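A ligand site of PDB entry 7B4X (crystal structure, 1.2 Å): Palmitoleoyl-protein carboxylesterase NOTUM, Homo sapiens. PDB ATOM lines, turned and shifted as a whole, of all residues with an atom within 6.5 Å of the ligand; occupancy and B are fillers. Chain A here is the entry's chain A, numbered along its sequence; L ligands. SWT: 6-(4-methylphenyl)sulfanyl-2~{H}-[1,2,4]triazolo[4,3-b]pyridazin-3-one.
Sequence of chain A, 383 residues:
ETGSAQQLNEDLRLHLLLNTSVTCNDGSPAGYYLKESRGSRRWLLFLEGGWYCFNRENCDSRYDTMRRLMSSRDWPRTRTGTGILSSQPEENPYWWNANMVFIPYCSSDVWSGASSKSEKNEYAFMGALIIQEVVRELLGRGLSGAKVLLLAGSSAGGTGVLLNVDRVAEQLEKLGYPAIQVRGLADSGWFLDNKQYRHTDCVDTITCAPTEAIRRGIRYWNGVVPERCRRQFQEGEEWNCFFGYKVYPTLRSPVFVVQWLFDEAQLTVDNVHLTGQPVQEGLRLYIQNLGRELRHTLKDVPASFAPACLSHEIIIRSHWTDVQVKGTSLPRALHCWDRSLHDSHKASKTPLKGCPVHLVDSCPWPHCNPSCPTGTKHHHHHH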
ATOM      1  N   GLY A  49       7.849  -0.773  15.785  1.00  0.00           N
ATOM      2  CA  GLY A  49       7.260  -2.093  15.763  1.00  0.00           C
ATOM      3  C   GLY A  49       7.087  -2.620  14.352  1.00  0.00           C
ATOM      4  O   GLY A  49       7.598  -2.070  13.377  1.00  0.00           O
ATOM      5  N   GLY A  50       6.356  -3.737  14.252  1.00  0.00           N
ATOM      6  CA  GLY A  50       6.124  -4.368  12.973  1.00  0.00           C
ATOM      7  C   GLY A  50       6.195  -5.880  12.991  1.00  0.00           C
ATOM      8  O   GLY A  50       6.806  -6.486  12.111  1.00  0.00           O
ATOM      9  N   TRP A  51       5.554  -6.505  13.992  1.00  0.00           N
ATOM     10  CA  TRP A  51       5.517  -7.960  14.117  1.00  0.00           C
ATOM     11  C   TRP A  51       6.910  -8.583  14.105  1.00  0.00           C
ATOM     12  O   TRP A  51       7.824  -8.062  14.746  1.00  0.00           O
ATOM     13  CB  TRP A  51       4.568  -8.587  13.093  1.00  0.00           C
ATOM     14  CG  TRP A  51       3.141  -8.251  13.361  1.00  0.00           C
ATOM     15  CD1 TRP A  51       2.386  -7.287  12.756  1.00  0.00           C
ATOM     16  CD2 TRP A  51       2.277  -8.866  14.334  1.00  0.00           C
ATOM     17  NE1 TRP A  51       1.117  -7.273  13.282  1.00  0.00           N
ATOM     18  CE2 TRP A  51       1.025  -8.230  14.249  1.00  0.00           C
ATOM     19  CE3 TRP A  51       2.456  -9.896  15.262  1.00  0.00           C
ATOM     20  CZ2 TRP A  51      -0.047  -8.592  15.060  1.00  0.00           C
ATOM     21  CZ3 TRP A  51       1.392 -10.257  16.068  1.00  0.00           C
ATOM     22  CH2 TRP A  51       0.149  -9.603  15.963  1.00  0.00           C
ATOM     23  N   TYR A  52       7.087  -9.681  13.372  1.00  0.00           N
ATOM     24  CA  TYR A  52       8.337 -10.435  13.358  1.00  0.00           C
ATOM     25  C   TYR A  52       8.202 -11.532  12.309  1.00  0.00           C
ATOM     26  O   TYR A  52       7.138 -11.714  11.701  1.00  0.00           O
ATOM     27  CB  TYR A  52       8.642 -11.023  14.744  1.00  0.00           C
ATOM     28  CG  TYR A  52       7.592 -11.981  15.254  1.00  0.00           C
ATOM     29  CD1 TYR A  52       7.667 -13.344  14.988  1.00  0.00           C
ATOM     30  CD2 TYR A  52       6.513 -11.523  16.006  1.00  0.00           C
ATOM     31  CE1 TYR A  52       6.709 -14.216  15.444  1.00  0.00           C
ATOM     32  CE2 TYR A  52       5.553 -12.397  16.479  1.00  0.00           C
ATOM     33  CZ  TYR A  52       5.645 -13.740  16.189  1.00  0.00           C
ATOM     34  OH  TYR A  52       4.691 -14.620  16.651  1.00  0.00           O
ATOM     35  N   TYR A 105      12.960  -0.602  12.958  1.00  0.00           N
ATOM     36  CA  TYR A 105      12.890  -2.032  13.252  1.00  0.00           C
ATOM     37  C   TYR A 105      13.222  -2.781  11.970  1.00  0.00           C
ATOM     38  O   TYR A 105      12.412  -2.826  11.043  1.00  0.00           O
ATOM     39  CB  TYR A 105      11.466  -2.346  13.713  1.00  0.00           C
ATOM     40  CG  TYR A 105      11.192  -3.772  14.122  1.00  0.00           C
ATOM     41  CD1 TYR A 105      12.122  -4.525  14.826  1.00  0.00           C
ATOM     42  CD2 TYR A 105       9.968  -4.360  13.808  1.00  0.00           C
ATOM     43  CE1 TYR A 105      11.838  -5.826  15.204  1.00  0.00           C
ATOM     44  CE2 TYR A 105       9.680  -5.654  14.181  1.00  0.00           C
ATOM     45  CZ  TYR A 105      10.613  -6.384  14.876  1.00  0.00           C
ATOM     46  OH  TYR A 105      10.309  -7.680  15.241  1.00  0.00           O
ATOM     47  N   VAL A 110      11.546  -8.964  17.403  1.00  0.00           N
ATOM     48  CA  VAL A 110      10.948  -8.294  18.558  1.00  0.00           C
ATOM     49  C   VAL A 110      12.090  -7.716  19.401  1.00  0.00           C
ATOM     50  O   VAL A 110      12.030  -7.675  20.638  1.00  0.00           O
ATOM     51  CB  VAL A 110      10.016  -9.250  19.341  1.00  0.00           C
ATOM     52  CG1 VAL A 110       9.313  -8.555  20.503  1.00  0.00           C
ATOM     53  CG2 VAL A 110       9.010  -9.909  18.393  1.00  0.00           C
ATOM     54  N   SER A 154       6.623   0.990  20.357  1.00  0.00           N
ATOM     55  CA  SER A 154       5.241   0.593  20.108  1.00  0.00           C
ATOM     56  C   SER A 154       5.159  -0.790  19.484  1.00  0.00           C
ATOM     57  O   SER A 154       5.993  -1.154  18.631  1.00  0.00           O
ATOM     58  CB  SER A 154       4.512   1.609  19.219  1.00  0.00           C
ATOM     59  OG  SER A 154       4.497   2.893  19.811  1.00  0.00           O
ATOM     60  N   SER A 155       4.148  -1.552  19.908  1.00  0.00           N
ATOM     61  CA  SER A 155       3.894  -2.929  19.487  1.00  0.00           C
ATOM     62  C   SER A 155       5.109  -3.828  19.678  1.00  0.00           C
ATOM     63  O   SER A 155       5.530  -4.072  20.815  1.00  0.00           O
ATOM     64  CB  SER A 155       3.313  -3.024  18.071  1.00  0.00           C
ATOM     65  OG  SER A 155       4.222  -2.609  17.076  1.00  0.00           O
ATOM     66  N   ALA A 156       5.691  -4.334  18.585  1.00  0.00           N
ATOM     67  CA  ALA A 156       6.926  -5.101  18.714  1.00  0.00           C
ATOM     68  C   ALA A 156       8.007  -4.294  19.428  1.00  0.00           C
ATOM     69  O   ALA A 156       8.800  -4.866  20.186  1.00  0.00           O
ATOM     70  CB  ALA A 156       7.418  -5.560  17.334  1.00  0.00           C
ATOM     71  N   GLY A 157       8.034  -2.975  19.225  1.00  0.00           N
ATOM     72  CA  GLY A 157       8.967  -2.137  19.953  1.00  0.00           C
ATOM     73  C   GLY A 157       8.583  -1.950  21.404  1.00  0.00           C
ATOM     74  O   GLY A 157       9.454  -1.727  22.257  1.00  0.00           O
ATOM     75  N   THR A 159       7.171  -4.387  23.332  1.00  0.00           N
ATOM     76  CA  THR A 159       7.754  -5.573  23.932  1.00  0.00           C
ATOM     77  C   THR A 159       9.281  -5.465  23.960  1.00  0.00           C
ATOM     78  O   THR A 159       9.928  -5.883  24.926  1.00  0.00           O
ATOM     79  CB  THR A 159       7.320  -6.815  23.153  1.00  0.00           C
ATOM     80  OG1 THR A 159       5.889  -6.816  23.022  1.00  0.00           O
ATOM     81  CG2 THR A 159       7.758  -8.076  23.882  1.00  0.00           C
ATOM     82  N   SER A 188       1.628  -0.654  23.731  1.00  0.00           N
ATOM     83  CA  SER A 188       0.962  -1.662  22.914  1.00  0.00           C
ATOM     84  C   SER A 188       1.804  -2.934  22.754  1.00  0.00           C
ATOM     85  O   SER A 188       1.739  -3.603  21.714  1.00  0.00           O
ATOM     86  CB  SER A 188       0.526  -1.092  21.556  1.00  0.00           C
ATOM     87  OG  SER A 188      -0.326   0.024  21.741  1.00  0.00           O
ATOM     88  N   GLY A 189       2.580  -3.288  23.774  1.00  0.00           N
ATOM     89  CA  GLY A 189       3.389  -4.486  23.737  1.00  0.00           C
ATOM     90  C   GLY A 189       3.133  -5.414  24.911  1.00  0.00           C
ATOM     91  O   GLY A 189       3.966  -6.274  25.223  1.00  0.00           O
ATOM     92  N   PHE A 191       0.848  -8.200  26.262  1.00  0.00           N
ATOM     93  CA  PHE A 191      -0.081  -9.187  25.701  1.00  0.00           C
ATOM     94  C   PHE A 191      -0.375 -10.302  26.697  1.00  0.00           C
ATOM     95  O   PHE A 191       0.361 -10.518  27.655  1.00  0.00           O
ATOM     96  CB  PHE A 191       0.465  -9.768  24.393  1.00  0.00           C
ATOM     97  CG  PHE A 191       0.703  -8.727  23.345  1.00  0.00           C
ATOM     98  CD1 PHE A 191      -0.376  -8.052  22.788  1.00  0.00           C
ATOM     99  CD2 PHE A 191       1.980  -8.407  22.936  1.00  0.00           C
ATOM    100  CE1 PHE A 191      -0.171  -7.077  21.826  1.00  0.00           C
ATOM    101  CE2 PHE A 191       2.184  -7.440  21.967  1.00  0.00           C
ATOM    102  CZ  PHE A 191       1.109  -6.771  21.416  1.00  0.00           C
ATOM    103  N   ILE A 214       6.358 -17.620  18.551  1.00  0.00           N
ATOM    104  CA  ILE A 214       7.395 -16.919  19.309  1.00  0.00           C
ATOM    105  C   ILE A 214       8.456 -17.901  19.810  1.00  0.00           C
ATOM    106  O   ILE A 214       9.657 -17.642  19.694  1.00  0.00           O
ATOM    107  CB  ILE A 214       6.772 -16.101  20.457  1.00  0.00           C
ATOM    108  CG1 ILE A 214       6.096 -14.849  19.908  1.00  0.00           C
ATOM    109  CG2 ILE A 214       7.826 -15.749  21.499  1.00  0.00           C
ATOM    110  CD1 ILE A 214       7.073 -13.740  19.545  1.00  0.00           C
ATOM    111  N   TRP A 239      10.233 -17.929  26.126  1.00  0.00           N
ATOM    112  CA  TRP A 239       9.084 -17.271  25.493  1.00  0.00           C
ATOM    113  C   TRP A 239       8.209 -16.574  26.522  1.00  0.00           C
ATOM    114  O   TRP A 239       7.532 -15.592  26.188  1.00  0.00           O
ATOM    115  CB  TRP A 239       8.280 -18.296  24.691  1.00  0.00           C
ATOM    116  CG  TRP A 239       7.602 -19.329  25.555  1.00  0.00           C
ATOM    117  CD1 TRP A 239       8.090 -20.557  25.884  1.00  0.00           C
ATOM    118  CD2 TRP A 239       6.324 -19.221  26.193  1.00  0.00           C
ATOM    119  NE1 TRP A 239       7.196 -21.221  26.688  1.00  0.00           N
ATOM    120  CE2 TRP A 239       6.103 -20.420  26.893  1.00  0.00           C
ATOM    121  CE3 TRP A 239       5.346 -18.218  26.240  1.00  0.00           C
ATOM    122  CZ2 TRP A 239       4.944 -20.645  27.641  1.00  0.00           C
ATOM    123  CZ3 TRP A 239       4.203 -18.445  26.973  1.00  0.00           C
ATOM    124  CH2 TRP A 239       4.012 -19.646  27.665  1.00  0.00           C
ATOM    125  N   PHE A 242       8.423 -12.767  26.890  1.00  0.00           N
ATOM    126  CA  PHE A 242       7.821 -11.871  25.908  1.00  0.00           C
ATOM    127  C   PHE A 242       6.448 -11.371  26.328  1.00  0.00           C
ATOM    128  O   PHE A 242       5.855 -10.556  25.618  1.00  0.00           O
ATOM    129  CB  PHE A 242       7.719 -12.558  24.543  1.00  0.00           C
ATOM    130  CG  PHE A 242       9.016 -12.583  23.778  1.00  0.00           C
ATOM    131  CD1 PHE A 242      10.140 -13.184  24.322  1.00  0.00           C
ATOM    132  CD2 PHE A 242       9.104 -12.018  22.522  1.00  0.00           C
ATOM    133  CE1 PHE A 242      11.337 -13.202  23.609  1.00  0.00           C
ATOM    134  CE2 PHE A 242      10.279 -12.033  21.813  1.00  0.00           C
ATOM    135  CZ  PHE A 242      11.405 -12.628  22.363  1.00  0.00           C
ATOM    136  N   PHE A 243       5.936 -11.837  27.450  1.00  0.00           N
ATOM    137  CA  PHE A 243       4.622 -11.445  27.940  1.00  0.00           C
ATOM    138  C   PHE A 243       4.811 -10.482  29.101  1.00  0.00           C
ATOM    139  O   PHE A 243       5.407 -10.843  30.127  1.00  0.00           O
ATOM    140  CB  PHE A 243       3.792 -12.666  28.295  1.00  0.00           C
ATOM    141  CG  PHE A 243       3.344 -13.429  27.093  1.00  0.00           C
ATOM    142  CD1 PHE A 243       2.171 -13.067  26.439  1.00  0.00           C
ATOM    143  CD2 PHE A 243       4.122 -14.431  26.567  1.00  0.00           C
ATOM    144  CE1 PHE A 243       1.774 -13.743  25.309  1.00  0.00           C
ATOM    145  CE2 PHE A 243       3.731 -15.111  25.425  1.00  0.00           C
ATOM    146  CZ  PHE A 243       2.552 -14.761  24.799  1.00  0.00           C
ATOM    147  N   ASP A 263      -6.836  -4.426  22.761  1.00  0.00           N
ATOM    148  CA  ASP A 263      -5.865  -4.174  21.704  1.00  0.00           C
ATOM    149  C   ASP A 263      -6.211  -5.010  20.470  1.00  0.00           C
ATOM    150  O   ASP A 263      -6.513  -6.196  20.574  1.00  0.00           O
ATOM    151  CB  ASP A 263      -4.474  -4.549  22.219  1.00  0.00           C
ATOM    152  CG  ASP A 263      -3.383  -4.275  21.204  1.00  0.00           C
ATOM    153  OD1 ASP A 263      -2.841  -3.156  21.204  1.00  0.00           O
ATOM    154  OD2 ASP A 263      -3.075  -5.201  20.424  1.00  0.00           O
ATOM    155  N   ALA A 265      -4.381  -6.101  18.029  1.00  0.00           N
ATOM    156  CA  ALA A 265      -3.479  -7.222  17.762  1.00  0.00           C
ATOM    157  C   ALA A 265      -3.775  -8.394  18.686  1.00  0.00           C
ATOM    158  O   ALA A 265      -3.709  -9.560  18.264  1.00  0.00           O
ATOM    159  CB  ALA A 265      -2.032  -6.778  17.892  1.00  0.00           C
ATOM    160  N   GLN A 266      -4.094  -8.116  19.946  1.00  0.00           N
ATOM    161  CA  GLN A 266      -4.524  -9.166  20.863  1.00  0.00           C
ATOM    162  C   GLN A 266      -5.781  -9.858  20.348  1.00  0.00           C
ATOM    163  O   GLN A 266      -5.853 -11.090  20.299  1.00  0.00           O
ATOM    164  CB  GLN A 266      -4.779  -8.568  22.251  1.00  0.00           C
ATOM    165  CG  GLN A 266      -5.274  -9.590  23.275  1.00  0.00           C
ATOM    166  CD  GLN A 266      -4.160 -10.442  23.848  1.00  0.00           C
ATOM    167  OE1 GLN A 266      -3.113  -9.916  24.260  1.00  0.00           O
ATOM    168  NE2 GLN A 266      -4.365 -11.746  23.866  1.00  0.00           N
ATOM    169  N   HIS A 312      -5.662  -0.027  17.453  1.00  0.00           N
ATOM    170  CA  HIS A 312      -4.266  -0.324  17.186  1.00  0.00           C
ATOM    171  C   HIS A 312      -3.412   0.947  17.188  1.00  0.00           C
ATOM    172  O   HIS A 312      -2.251   0.895  16.772  1.00  0.00           O
ATOM    173  CB  HIS A 312      -4.102  -1.028  15.842  1.00  0.00           C
ATOM    174  CG  HIS A 312      -4.500  -0.192  14.672  1.00  0.00           C
ATOM    175  ND1 HIS A 312      -5.720  -0.311  14.052  1.00  0.00           N
ATOM    176  CD2 HIS A 312      -3.830   0.780  14.010  1.00  0.00           C
ATOM    177  CE1 HIS A 312      -5.789   0.559  13.046  1.00  0.00           C
ATOM    178  NE2 HIS A 312      -4.651   1.231  13.009  1.00  0.00           N
HETATM  179  C17 SWT L   1       1.499  -6.899  18.041  1.00  0.00           C
HETATM  180  C01 SWT L   1       3.958 -11.977  22.853  1.00  0.00           C
HETATM  181  C02 SWT L   1       4.291 -11.092  21.654  1.00  0.00           C
HETATM  182  C03 SWT L   1       4.967  -9.886  21.842  1.00  0.00           C
HETATM  183  C04 SWT L   1       5.274  -9.082  20.758  1.00  0.00           C
HETATM  184  C05 SWT L   1       4.909  -9.476  19.476  1.00  0.00           C
HETATM  185  C06 SWT L   1       4.234 -10.675  19.296  1.00  0.00           C
HETATM  186  C07 SWT L   1       3.927 -11.478  20.380  1.00  0.00           C
HETATM  187  C09 SWT L   1       3.816  -7.478  17.636  1.00  0.00           C
HETATM  188  C12 SWT L   1       2.563  -4.871  15.236  1.00  0.00           C
HETATM  189  C16 SWT L   1       1.581  -6.006  16.981  1.00  0.00           C
HETATM  190  C18 SWT L   1       2.609  -7.652  18.380  1.00  0.00           C
HETATM  191  N10 SWT L   1       3.869  -6.609  16.623  1.00  0.00           N
HETATM  192  N11 SWT L   1       2.744  -5.873  16.291  1.00  0.00           N
HETATM  193  N14 SWT L   1       1.225  -4.405  15.311  1.00  0.00           N
HETATM  194  N15 SWT L   1       0.599  -5.077  16.366  1.00  0.00           N
HETATM  195  O13 SWT L   1       3.387  -4.533  14.466  1.00  0.00           O
HETATM  196  S08 SWT L   1       5.295  -8.439  18.047  1.00  0.00           S
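An oxygen (O13) of the ligand lies within hydrogen-bond range of the backbone NH (N) of Trp 51.
The backbone NH (N) of Gly 50 is in hydrogen-bond range of an oxygen (O13) of the ligand, 3.1 Å away.
The side-chain hydroxyl of Ser 155 lies within hydrogen-bond range of an oxygen (O13) of the ligand, 3.3 Å away.
The backbone carbonyl oxygen (O) of Trp 51 lies within hydrogen-bond range of the side-chain hydroxyl (OH) of Tyr 105, at 2.6 Å.
The backbone carbonyl oxygen of Gly 189 lies within hydrogen-bond range of the side-chain hydroxyl of Thr 159, at 3.0 Å.
N of Ala 265 sits at hydrogen-bond distance from OD2 of Asp 263 (2.9 Å).
Tyr 52 touches the ligand (CE2 to C06, 3.6 Å).
Ala 156 touches the ligand.
Thr 159 touches the ligand (OG1 to C04, 3.3 Å).
Phe 191 touches the ligand.
CD1 of Ile 214 touches C07 of the ligand (3.96 Å).
O of Phe 242 touches C01 of the ligand, at 3.6 Å.
Phe 243 touches the ligand (CZ to C01, 3.7 Å).
CB of Ala 265 touches N15 of the ligand (3.5 Å).
Hydrophobic or aromatic side chains within 4 Å of the ligand: Trp 51, Tyr 52, Ala 156, Phe 191, Ile 214, Phe 243 and Ala 265.
Of the 22 residues printed, 11 come within 4 Å of the ligand.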
